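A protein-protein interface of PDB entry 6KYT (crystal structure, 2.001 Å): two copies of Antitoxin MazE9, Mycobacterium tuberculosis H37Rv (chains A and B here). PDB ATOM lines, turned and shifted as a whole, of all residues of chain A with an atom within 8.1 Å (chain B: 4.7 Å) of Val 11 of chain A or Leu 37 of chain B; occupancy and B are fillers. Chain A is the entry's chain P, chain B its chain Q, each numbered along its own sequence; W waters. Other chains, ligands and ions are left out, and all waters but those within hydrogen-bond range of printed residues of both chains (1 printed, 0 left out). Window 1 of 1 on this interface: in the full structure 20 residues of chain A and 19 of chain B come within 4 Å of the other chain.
O of Val 11 of chain B is in hydrogen-bond range of N of Leu 9 of chain A (3.2 Å). OG of Ser 10 of chain A sits close to O of Leu 9 of chain B, 3.5 Å away. The backbone NH (N) of Leu 9 of chain B sits at hydrogen-bond distance from the backbone carbonyl oxygen (O) of Val 11 of chain A (2.9 Å). The backbone NH (N) of Ser 12 of chain A sits at hydrogen-bond distance from the side-chain hydroxyl (OG) of Ser 34 of chain B. O of Val 7 of chain B is in hydrogen-bond range of N of Leu 13 of chain A (2.7 Å). The side-chain carboxylate (OD1) of Asp 17 of chain A sits at hydrogen-bond distance from the side-chain amide nitrogen (NE2) of Gln 38 of chain B.
The side-chain hydroxyl (OG) of Ser 14 of chain A lies within hydrogen-bond range of the side-chain carboxylate (OD1) of Asp 17 of chain A (2.9 Å).
Among the printed residues, pairs that only touch across the chains: Val 11 of chain A with Lys 8 of chain B, Lys 8 of chain A with Val 11 of chain B, Ser 12 of chain A with Val 7 of chain B, Val 11 of chain A with Leu 37 of chain B, Val 11 of chain A with Ser 34 of chain B, Ser 12 of chain A with Lys 8 of chain B, Ala 40 of chain A with Ala 40 of chain B, Leu 44 of chain A with Ala 40 of chain B, Leu 13 of chain A with Ile 41 of chain B, Leu 9 of chain A with Leu 9 of chain B, Val 18 of chain A with Val 7 of chain B, Asp 17 of chain A with Ile 41 of chain B, Leu 37 of chain A with Val 11 of chain B, Leu 13 of chain A with Gln 38 of chain B, Leu 13 of chain A with Ser 34 of chain B, Val 11 of chain A with Val 7 of chain B, Ser 14 of chain A with Gln 38 of chain B, Leu 37 of chain A with Ile 41 of chain B and Ser 10 of chain A with Lys 8 of chain B.
Of the printed residues of chain B, Lys 8 of chain A touches Val 11 (3.4 Å). Val 11 of chain A touches five residues of chain B. Printed residues of chain B within 4 Å of Val 18 of chain A: Val 7 (3.7 Å). Gln 38 of chain A touches none of the printed residues of chain B. Printed residues of chain A within 4 Å of Val 11 of chain B: Lys 8, Leu 9 and Leu 37. Arg 33 of chain B touches none of the printed residues of chain A. No residue of chain A comes within 4 Å of Gly 36 of chain B. Leu 37 of chain B touches just one residue of chain A: Val 11 (3.4 Å). The nearest residue of chain B that does not touch Val 11 of chain A is Val 11 of chain B (4.6 Å). The nearest residue of chain A that does not touch Leu 37 of chain B is Ile 41 of chain A (4.1 Å). The nearest printed residue of chain B that does not touch Ser 14 of chain A is Val 7 of chain B (4.6 Å).
Of the 16 printed residues of chain A, 12 touch a printed residue of chain B. Hydrophobic or aromatic side chains of chain A that line the printed part of chain B: Leu 9, Val 11, Leu 13, Val 18, Leu 37, Ala 40 and Leu 44. Among the printed residues, no Asp or Glu carboxylate lies within 4 Å of a Lys or Arg side-chain nitrogen of the other chain.
Leu 9 of chain A touches its own counterpart, Leu 9 of chain B. Val 11 of chain A touches Leu 37 of chain B, and with the chains exchanged Leu 37 of chain A touches Val 11 of chain B. Leu 37 of chain A touches Ile 41 of chain B, but with the chains exchanged Ile 41 of chain A does not touch Leu 37 of chain B (4.1 Å). Ala 40 of chain A touches its own counterpart, Ala 40 of chain B.
Water W1 bridges the side-chain carboxylate of Asp 17 of chain A (2.5 Å) and the backbone carbonyl oxygen of Gln 38 of chain B (2.8 Å).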
ATOM      1  N   LYS A   8       8.596  19.701 -24.739  1.00  0.00           N
ATOM      2  CA  LYS A   8       7.456  20.079 -25.567  1.00  0.00           C
ATOM      3  C   LYS A   8       6.233  19.245 -25.220  1.00  0.00           C
ATOM      4  O   LYS A   8       6.316  18.022 -25.099  1.00  0.00           O
ATOM      5  CB  LYS A   8       7.784  19.920 -27.050  1.00  0.00           C
ATOM      6  CG  LYS A   8       9.022  20.670 -27.497  1.00  0.00           C
ATOM      7  CD  LYS A   8       9.256  20.498 -28.990  1.00  0.00           C
ATOM      8  CE  LYS A   8       8.187  21.206 -29.805  1.00  0.00           C
ATOM      9  NZ  LYS A   8       8.247  22.683 -29.625  1.00  0.00           N
ATOM     10  N   LEU A   9       5.096  19.914 -25.065  1.00  0.00           N
ATOM     11  CA  LEU A   9       3.840  19.284 -24.691  1.00  0.00           C
ATOM     12  C   LEU A   9       2.763  19.693 -25.681  1.00  0.00           C
ATOM     13  O   LEU A   9       2.967  20.568 -26.527  1.00  0.00           O
ATOM     14  CB  LEU A   9       3.424  19.659 -23.258  1.00  0.00           C
ATOM     15  CG  LEU A   9       3.333  21.154 -22.899  1.00  0.00           C
ATOM     16  CD1 LEU A   9       2.093  21.865 -23.458  1.00  0.00           C
ATOM     17  CD2 LEU A   9       3.421  21.340 -21.371  1.00  0.00           C
ATOM     18  N   SER A  10       1.602  19.052 -25.565  1.00  0.00           N
ATOM     19  CA  SER A  10       0.387  19.479 -26.250  1.00  0.00           C
ATOM     20  C   SER A  10      -0.669  19.814 -25.205  1.00  0.00           C
ATOM     21  O   SER A  10      -0.979  18.977 -24.350  1.00  0.00           O
ATOM     22  CB  SER A  10      -0.130  18.394 -27.204  1.00  0.00           C
ATOM     23  OG  SER A  10      -1.016  18.924 -28.183  1.00  0.00           O
ATOM     24  N   VAL A  11      -1.205  21.040 -25.262  1.00  0.00           N
ATOM     25  CA  VAL A  11      -2.298  21.470 -24.392  1.00  0.00           C
ATOM     26  C   VAL A  11      -3.557  21.749 -25.199  1.00  0.00           C
ATOM     27  O   VAL A  11      -3.514  22.050 -26.396  1.00  0.00           O
ATOM     28  CB  VAL A  11      -1.967  22.713 -23.536  1.00  0.00           C
ATOM     29  CG1 VAL A  11      -0.850  22.408 -22.569  1.00  0.00           C
ATOM     30  CG2 VAL A  11      -1.605  23.889 -24.427  1.00  0.00           C
ATOM     31  N   SER A  12      -4.687  21.675 -24.497  1.00  0.00           N
ATOM     32  CA  SER A  12      -6.012  21.961 -25.032  1.00  0.00           C
ATOM     33  C   SER A  12      -6.578  23.163 -24.288  1.00  0.00           C
ATOM     34  O   SER A  12      -6.770  23.108 -23.068  1.00  0.00           O
ATOM     35  CB  SER A  12      -6.928  20.745 -24.883  1.00  0.00           C
ATOM     36  OG  SER A  12      -6.232  19.574 -25.268  1.00  0.00           O
ATOM     37  N   LEU A  13      -6.816  24.251 -25.017  1.00  0.00           N
ATOM     38  CA  LEU A  13      -7.372  25.475 -24.462  1.00  0.00           C
ATOM     39  C   LEU A  13      -8.568  25.899 -25.299  1.00  0.00           C
ATOM     40  O   LEU A  13      -8.794  25.399 -26.403  1.00  0.00           O
ATOM     41  CB  LEU A  13      -6.334  26.605 -24.419  1.00  0.00           C
ATOM     42  CG  LEU A  13      -4.966  26.272 -23.830  1.00  0.00           C
ATOM     43  CD1 LEU A  13      -3.982  27.387 -24.138  1.00  0.00           C
ATOM     44  CD2 LEU A  13      -5.074  26.040 -22.332  1.00  0.00           C
ATOM     45  N   SER A  14      -9.339  26.839 -24.761  1.00  0.00           N
ATOM     46  CA  SER A  14     -10.477  27.361 -25.492  1.00  0.00           C
ATOM     47  C   SER A  14     -10.039  28.485 -26.428  1.00  0.00           C
ATOM     48  O   SER A  14      -8.959  29.072 -26.289  1.00  0.00           O
ATOM     49  CB  SER A  14     -11.553  27.860 -24.530  1.00  0.00           C
ATOM     50  OG  SER A  14     -11.146  29.056 -23.889  1.00  0.00           O
ATOM     51  N   ASP A  17      -9.296  31.450 -24.509  1.00  0.00           N
ATOM     52  CA  ASP A  17      -7.982  31.345 -23.882  1.00  0.00           C
ATOM     53  C   ASP A  17      -6.881  31.737 -24.860  1.00  0.00           C
ATOM     54  O   ASP A  17      -5.998  32.541 -24.534  1.00  0.00           O
ATOM     55  CB  ASP A  17      -7.754  29.926 -23.360  1.00  0.00           C
ATOM     56  CG  ASP A  17      -8.673  29.572 -22.210  1.00  0.00           C
ATOM     57  OD1 ASP A  17      -8.976  28.374 -22.038  1.00  0.00           O
ATOM     58  OD2 ASP A  17      -9.095  30.493 -21.479  1.00  0.00           O
ATOM     59  N   VAL A  18      -6.920  31.181 -26.073  1.00  0.00           N
ATOM     60  CA  VAL A  18      -5.868  31.501 -27.033  1.00  0.00           C
ATOM     61  C   VAL A  18      -5.958  32.960 -27.467  1.00  0.00           C
ATOM     62  O   VAL A  18      -4.938  33.582 -27.782  1.00  0.00           O
ATOM     63  CB  VAL A  18      -5.917  30.540 -28.236  1.00  0.00           C
ATOM     64  CG1 VAL A  18      -4.673  30.714 -29.096  1.00  0.00           C
ATOM     65  CG2 VAL A  18      -6.026  29.101 -27.757  1.00  0.00           C
ATOM     66  N   LEU A  21      -4.279  34.915 -24.639  1.00  0.00           N
ATOM     67  CA  LEU A  21      -2.838  34.695 -24.717  1.00  0.00           C
ATOM     68  C   LEU A  21      -2.220  35.485 -25.865  1.00  0.00           C
ATOM     69  O   LEU A  21      -1.171  36.121 -25.704  1.00  0.00           O
ATOM     70  CB  LEU A  21      -2.551  33.201 -24.872  1.00  0.00           C
ATOM     71  CG  LEU A  21      -1.100  32.781 -25.117  1.00  0.00           C
ATOM     72  CD1 LEU A  21      -0.238  33.049 -23.892  1.00  0.00           C
ATOM     73  CD2 LEU A  21      -1.037  31.315 -25.515  1.00  0.00           C
ATOM     74  N   GLY A  36       4.535  33.753 -23.791  1.00  0.00           N
ATOM     75  CA  GLY A  36       3.388  34.195 -23.007  1.00  0.00           C
ATOM     76  C   GLY A  36       3.090  33.269 -21.841  1.00  0.00           C
ATOM     77  O   GLY A  36       2.935  33.715 -20.697  1.00  0.00           O
ATOM     78  N   LEU A  37       3.031  31.964 -22.113  1.00  0.00           N
ATOM     79  CA  LEU A  37       2.741  30.991 -21.066  1.00  0.00           C
ATOM     80  C   LEU A  37       3.838  30.967 -20.011  1.00  0.00           C
ATOM     81  O   LEU A  37       3.569  30.713 -18.830  1.00  0.00           O
ATOM     82  CB  LEU A  37       2.560  29.603 -21.680  1.00  0.00           C
ATOM     83  CG  LEU A  37       1.372  29.428 -22.626  1.00  0.00           C
ATOM     84  CD1 LEU A  37       1.330  28.014 -23.184  1.00  0.00           C
ATOM     85  CD2 LEU A  37       0.076  29.759 -21.906  1.00  0.00           C
ATOM     86  N   GLN A  38       5.084  31.218 -20.420  1.00  0.00           N
ATOM     87  CA  GLN A  38       6.171  31.312 -19.453  1.00  0.00           C
ATOM     88  C   GLN A  38       5.949  32.475 -18.498  1.00  0.00           C
ATOM     89  O   GLN A  38       6.149  32.339 -17.283  1.00  0.00           O
ATOM     90  CB  GLN A  38       7.511  31.457 -20.176  1.00  0.00           C
ATOM     91  N   ALA A  40       3.020  33.693 -17.695  1.00  0.00           N
ATOM     92  CA  ALA A  40       1.908  33.289 -16.835  1.00  0.00           C
ATOM     93  C   ALA A  40       2.378  32.379 -15.704  1.00  0.00           C
ATOM     94  O   ALA A  40       2.030  32.587 -14.534  1.00  0.00           O
ATOM     95  CB  ALA A  40       0.832  32.591 -17.664  1.00  0.00           C
ATOM     96  N   ILE A  41       3.166  31.355 -16.042  1.00  0.00           N
ATOM     97  CA  ILE A  41       3.657  30.418 -15.036  1.00  0.00           C
ATOM     98  C   ILE A  41       4.524  31.140 -14.013  1.00  0.00           C
ATOM     99  O   ILE A  41       4.438  30.877 -12.807  1.00  0.00           O
ATOM    100  CB  ILE A  41       4.416  29.263 -15.715  1.00  0.00           C
ATOM    101  CG1 ILE A  41       3.452  28.411 -16.543  1.00  0.00           C
ATOM    102  CG2 ILE A  41       5.140  28.408 -14.686  1.00  0.00           C
ATOM    103  CD1 ILE A  41       4.140  27.405 -17.436  1.00  0.00           C
ATOM    104  N   LEU A  44       2.164  32.694 -11.606  1.00  0.00           N
ATOM    105  CA  LEU A  44       1.687  31.677 -10.669  1.00  0.00           C
ATOM    106  C   LEU A  44       2.750  31.328  -9.638  1.00  0.00           C
ATOM    107  O   LEU A  44       2.426  30.905  -8.522  1.00  0.00           O
ATOM    108  CB  LEU A  44       1.278  30.406 -11.416  1.00  0.00           C
ATOM    109  CG  LEU A  44       0.089  30.411 -12.370  1.00  0.00           C
ATOM    110  CD1 LEU A  44      -0.146  29.001 -12.889  1.00  0.00           C
ATOM    111  CD2 LEU A  44      -1.151  30.942 -11.677  1.00  0.00           C
ATOM    112  N   VAL B   7      -9.089  24.452 -28.953  1.00  0.00           N
ATOM    113  CA  VAL B   7      -7.834  24.691 -29.656  1.00  0.00           C
ATOM    114  C   VAL B   7      -6.714  23.934 -28.957  1.00  0.00           C
ATOM    115  O   VAL B   7      -6.625  23.922 -27.723  1.00  0.00           O
ATOM    116  CB  VAL B   7      -7.534  26.199 -29.725  1.00  0.00           C
ATOM    117  CG1 VAL B   7      -6.173  26.448 -30.361  1.00  0.00           C
ATOM    118  CG2 VAL B   7      -8.626  26.924 -30.493  1.00  0.00           C
ATOM    119  N   LYS B   8      -5.859  23.291 -29.746  1.00  0.00           N
ATOM    120  CA  LYS B   8      -4.703  22.580 -29.228  1.00  0.00           C
ATOM    121  C   LYS B   8      -3.420  23.268 -29.679  1.00  0.00           C
ATOM    122  O   LYS B   8      -3.333  23.791 -30.793  1.00  0.00           O
ATOM    123  CB  LYS B   8      -4.703  21.117 -29.682  1.00  0.00           C
ATOM    124  CG  LYS B   8      -5.924  20.335 -29.227  1.00  0.00           C
ATOM    125  CD  LYS B   8      -5.530  18.992 -28.634  1.00  0.00           C
ATOM    126  CE  LYS B   8      -4.666  18.200 -29.594  1.00  0.00           C
ATOM    127  NZ  LYS B   8      -4.456  16.797 -29.138  1.00  0.00           N
ATOM    128  N   LEU B   9      -2.424  23.267 -28.794  1.00  0.00           N
ATOM    129  CA  LEU B   9      -1.150  23.917 -29.055  1.00  0.00           C
ATOM    130  C   LEU B   9      -0.008  22.991 -28.674  1.00  0.00           C
ATOM    131  O   LEU B   9      -0.111  22.231 -27.708  1.00  0.00           O
ATOM    132  CB  LEU B   9      -1.000  25.223 -28.261  1.00  0.00           C
ATOM    133  CG  LEU B   9      -2.003  26.363 -28.432  1.00  0.00           C
ATOM    134  CD1 LEU B   9      -1.518  27.582 -27.665  1.00  0.00           C
ATOM    135  CD2 LEU B   9      -2.209  26.698 -29.896  1.00  0.00           C
ATOM    136  N   VAL B  11       3.599  23.649 -27.247  1.00  0.00           N
ATOM    137  CA  VAL B  11       4.365  24.728 -26.643  1.00  0.00           C
ATOM    138  C   VAL B  11       5.625  24.152 -26.010  1.00  0.00           C
ATOM    139  O   VAL B  11       5.707  22.964 -25.689  1.00  0.00           O
ATOM    140  CB  VAL B  11       3.550  25.525 -25.595  1.00  0.00           C
ATOM    141  CG1 VAL B  11       2.156  25.845 -26.121  1.00  0.00           C
ATOM    142  CG2 VAL B  11       3.477  24.780 -24.289  1.00  0.00           C
ATOM    143  N   LEU B  21       4.189  24.372 -12.983  1.00  0.00           N
ATOM    144  CA  LEU B  21       2.820  24.134 -13.430  1.00  0.00           C
ATOM    145  C   LEU B  21       2.216  22.912 -12.751  1.00  0.00           C
ATOM    146  O   LEU B  21       1.069  22.953 -12.288  1.00  0.00           O
ATOM    147  CB  LEU B  21       2.793  23.976 -14.950  1.00  0.00           C
ATOM    148  CG  LEU B  21       1.455  23.594 -15.586  1.00  0.00           C
ATOM    149  CD1 LEU B  21       0.374  24.597 -15.211  1.00  0.00           C
ATOM    150  CD2 LEU B  21       1.600  23.493 -17.096  1.00  0.00           C
ATOM    151  N   ARG B  33      -2.556  19.603 -16.708  1.00  0.00           N
ATOM    152  CA  ARG B  33      -1.717  20.745 -17.052  1.00  0.00           C
ATOM    153  C   ARG B  33      -2.465  21.761 -17.903  1.00  0.00           C
ATOM    154  O   ARG B  33      -2.230  22.965 -17.773  1.00  0.00           O
ATOM    155  CB  ARG B  33      -0.461  20.263 -17.786  1.00  0.00           C
ATOM    156  CG  ARG B  33       0.447  19.383 -16.939  1.00  0.00           C
ATOM    157  CD  ARG B  33       1.602  18.801 -17.743  1.00  0.00           C
ATOM    158  NE  ARG B  33       2.637  18.251 -16.870  1.00  0.00           N
ATOM    159  CZ  ARG B  33       3.660  17.512 -17.291  1.00  0.00           C
ATOM    160  NH1 ARG B  33       3.791  17.229 -18.580  1.00  0.00           N
ATOM    161  NH2 ARG B  33       4.552  17.057 -16.422  1.00  0.00           N
ATOM    162  N   SER B  34      -3.364  21.301 -18.779  1.00  0.00           N
ATOM    163  CA  SER B  34      -4.146  22.228 -19.592  1.00  0.00           C
ATOM    164  C   SER B  34      -5.036  23.110 -18.723  1.00  0.00           C
ATOM    165  O   SER B  34      -5.107  24.329 -18.929  1.00  0.00           O
ATOM    166  CB  SER B  34      -4.984  21.457 -20.612  1.00  0.00           C
ATOM    167  OG  SER B  34      -4.157  20.797 -21.557  1.00  0.00           O
ATOM    168  N   ALA B  35      -5.730  22.515 -17.751  1.00  0.00           N
ATOM    169  CA  ALA B  35      -6.519  23.314 -16.817  1.00  0.00           C
ATOM    170  C   ALA B  35      -5.626  24.274 -16.039  1.00  0.00           C
ATOM    171  O   ALA B  35      -5.964  25.457 -15.867  1.00  0.00           O
ATOM    172  CB  ALA B  35      -7.293  22.399 -15.868  1.00  0.00           C
ATOM    173  N   GLY B  36      -4.471  23.784 -15.577  1.00  0.00           N
ATOM    174  CA  GLY B  36      -3.499  24.673 -14.960  1.00  0.00           C
ATOM    175  C   GLY B  36      -3.173  25.871 -15.832  1.00  0.00           C
ATOM    176  O   GLY B  36      -3.084  27.003 -15.347  1.00  0.00           O
ATOM    177  N   LEU B  37      -3.029  25.642 -17.138  1.00  0.00           N
ATOM    178  CA  LEU B  37      -2.653  26.723 -18.042  1.00  0.00           C
ATOM    179  C   LEU B  37      -3.822  27.652 -18.339  1.00  0.00           C
ATOM    180  O   LEU B  37      -3.607  28.831 -18.639  1.00  0.00           O
ATOM    181  CB  LEU B  37      -2.078  26.152 -19.337  1.00  0.00           C
ATOM    182  CG  LEU B  37      -0.662  25.595 -19.184  1.00  0.00           C
ATOM    183  CD1 LEU B  37      -0.155  25.037 -20.489  1.00  0.00           C
ATOM    184  CD2 LEU B  37       0.273  26.679 -18.690  1.00  0.00           C
ATOM    185  N   GLN B  38      -5.058  27.152 -18.271  1.00  0.00           N
ATOM    186  CA  GLN B  38      -6.210  28.043 -18.352  1.00  0.00           C
ATOM    187  C   GLN B  38      -6.215  29.015 -17.177  1.00  0.00           C
ATOM    188  O   GLN B  38      -6.372  30.235 -17.357  1.00  0.00           O
ATOM    189  CB  GLN B  38      -7.507  27.233 -18.394  1.00  0.00           C
ATOM    190  CG  GLN B  38      -7.757  26.517 -19.715  1.00  0.00           C
ATOM    191  CD  GLN B  38      -9.140  25.897 -19.789  1.00  0.00           C
ATOM    192  OE1 GLN B  38      -9.661  25.389 -18.796  1.00  0.00           O
ATOM    193  NE2 GLN B  38      -9.749  25.945 -20.969  1.00  0.00           N
ATOM    194  N   HIS B  39      -6.026  28.487 -15.961  1.00  0.00           N
ATOM    195  CA  HIS B  39      -5.894  29.361 -14.798  1.00  0.00           C
ATOM    196  C   HIS B  39      -4.767  30.372 -14.991  1.00  0.00           C
ATOM    197  O   HIS B  39      -4.934  31.570 -14.709  1.00  0.00           O
ATOM    198  CB  HIS B  39      -5.654  28.527 -13.538  1.00  0.00           C
ATOM    199  CG  HIS B  39      -6.881  27.845 -13.020  1.00  0.00           C
ATOM    200  ND1 HIS B  39      -7.239  27.867 -11.689  1.00  0.00           N
ATOM    201  CD2 HIS B  39      -7.838  27.124 -13.654  1.00  0.00           C
ATOM    202  CE1 HIS B  39      -8.361  27.187 -11.524  1.00  0.00           C
ATOM    203  NE2 HIS B  39      -8.745  26.728 -12.702  1.00  0.00           N
ATOM    204  N   ALA B  40      -3.617  29.910 -15.493  1.00  0.00           N
ATOM    205  CA  ALA B  40      -2.484  30.808 -15.694  1.00  0.00           C
ATOM    206  C   ALA B  40      -2.817  31.920 -16.683  1.00  0.00           C
ATOM    207  O   ALA B  40      -2.439  33.079 -16.475  1.00  0.00           O
ATOM    208  CB  ALA B  40      -1.269  30.017 -16.173  1.00  0.00           C
ATOM    209  N   ILE B  41      -3.524  31.586 -17.768  1.00  0.00           N
ATOM    210  CA  ILE B  41      -3.871  32.592 -18.769  1.00  0.00           C
ATOM    211  C   ILE B  41      -4.810  33.632 -18.177  1.00  0.00           C
ATOM    212  O   ILE B  41      -4.656  34.835 -18.422  1.00  0.00           O
ATOM    213  CB  ILE B  41      -4.480  31.925 -20.017  1.00  0.00           C
ATOM    214  CG1 ILE B  41      -3.424  31.092 -20.741  1.00  0.00           C
ATOM    215  CG2 ILE B  41      -5.062  32.972 -20.957  1.00  0.00           C
ATOM    216  CD1 ILE B  41      -4.002  30.118 -21.736  1.00  0.00           C
HETATM  217  O   HOH W   1      -8.242  31.241 -19.208  1.00  0.00           O
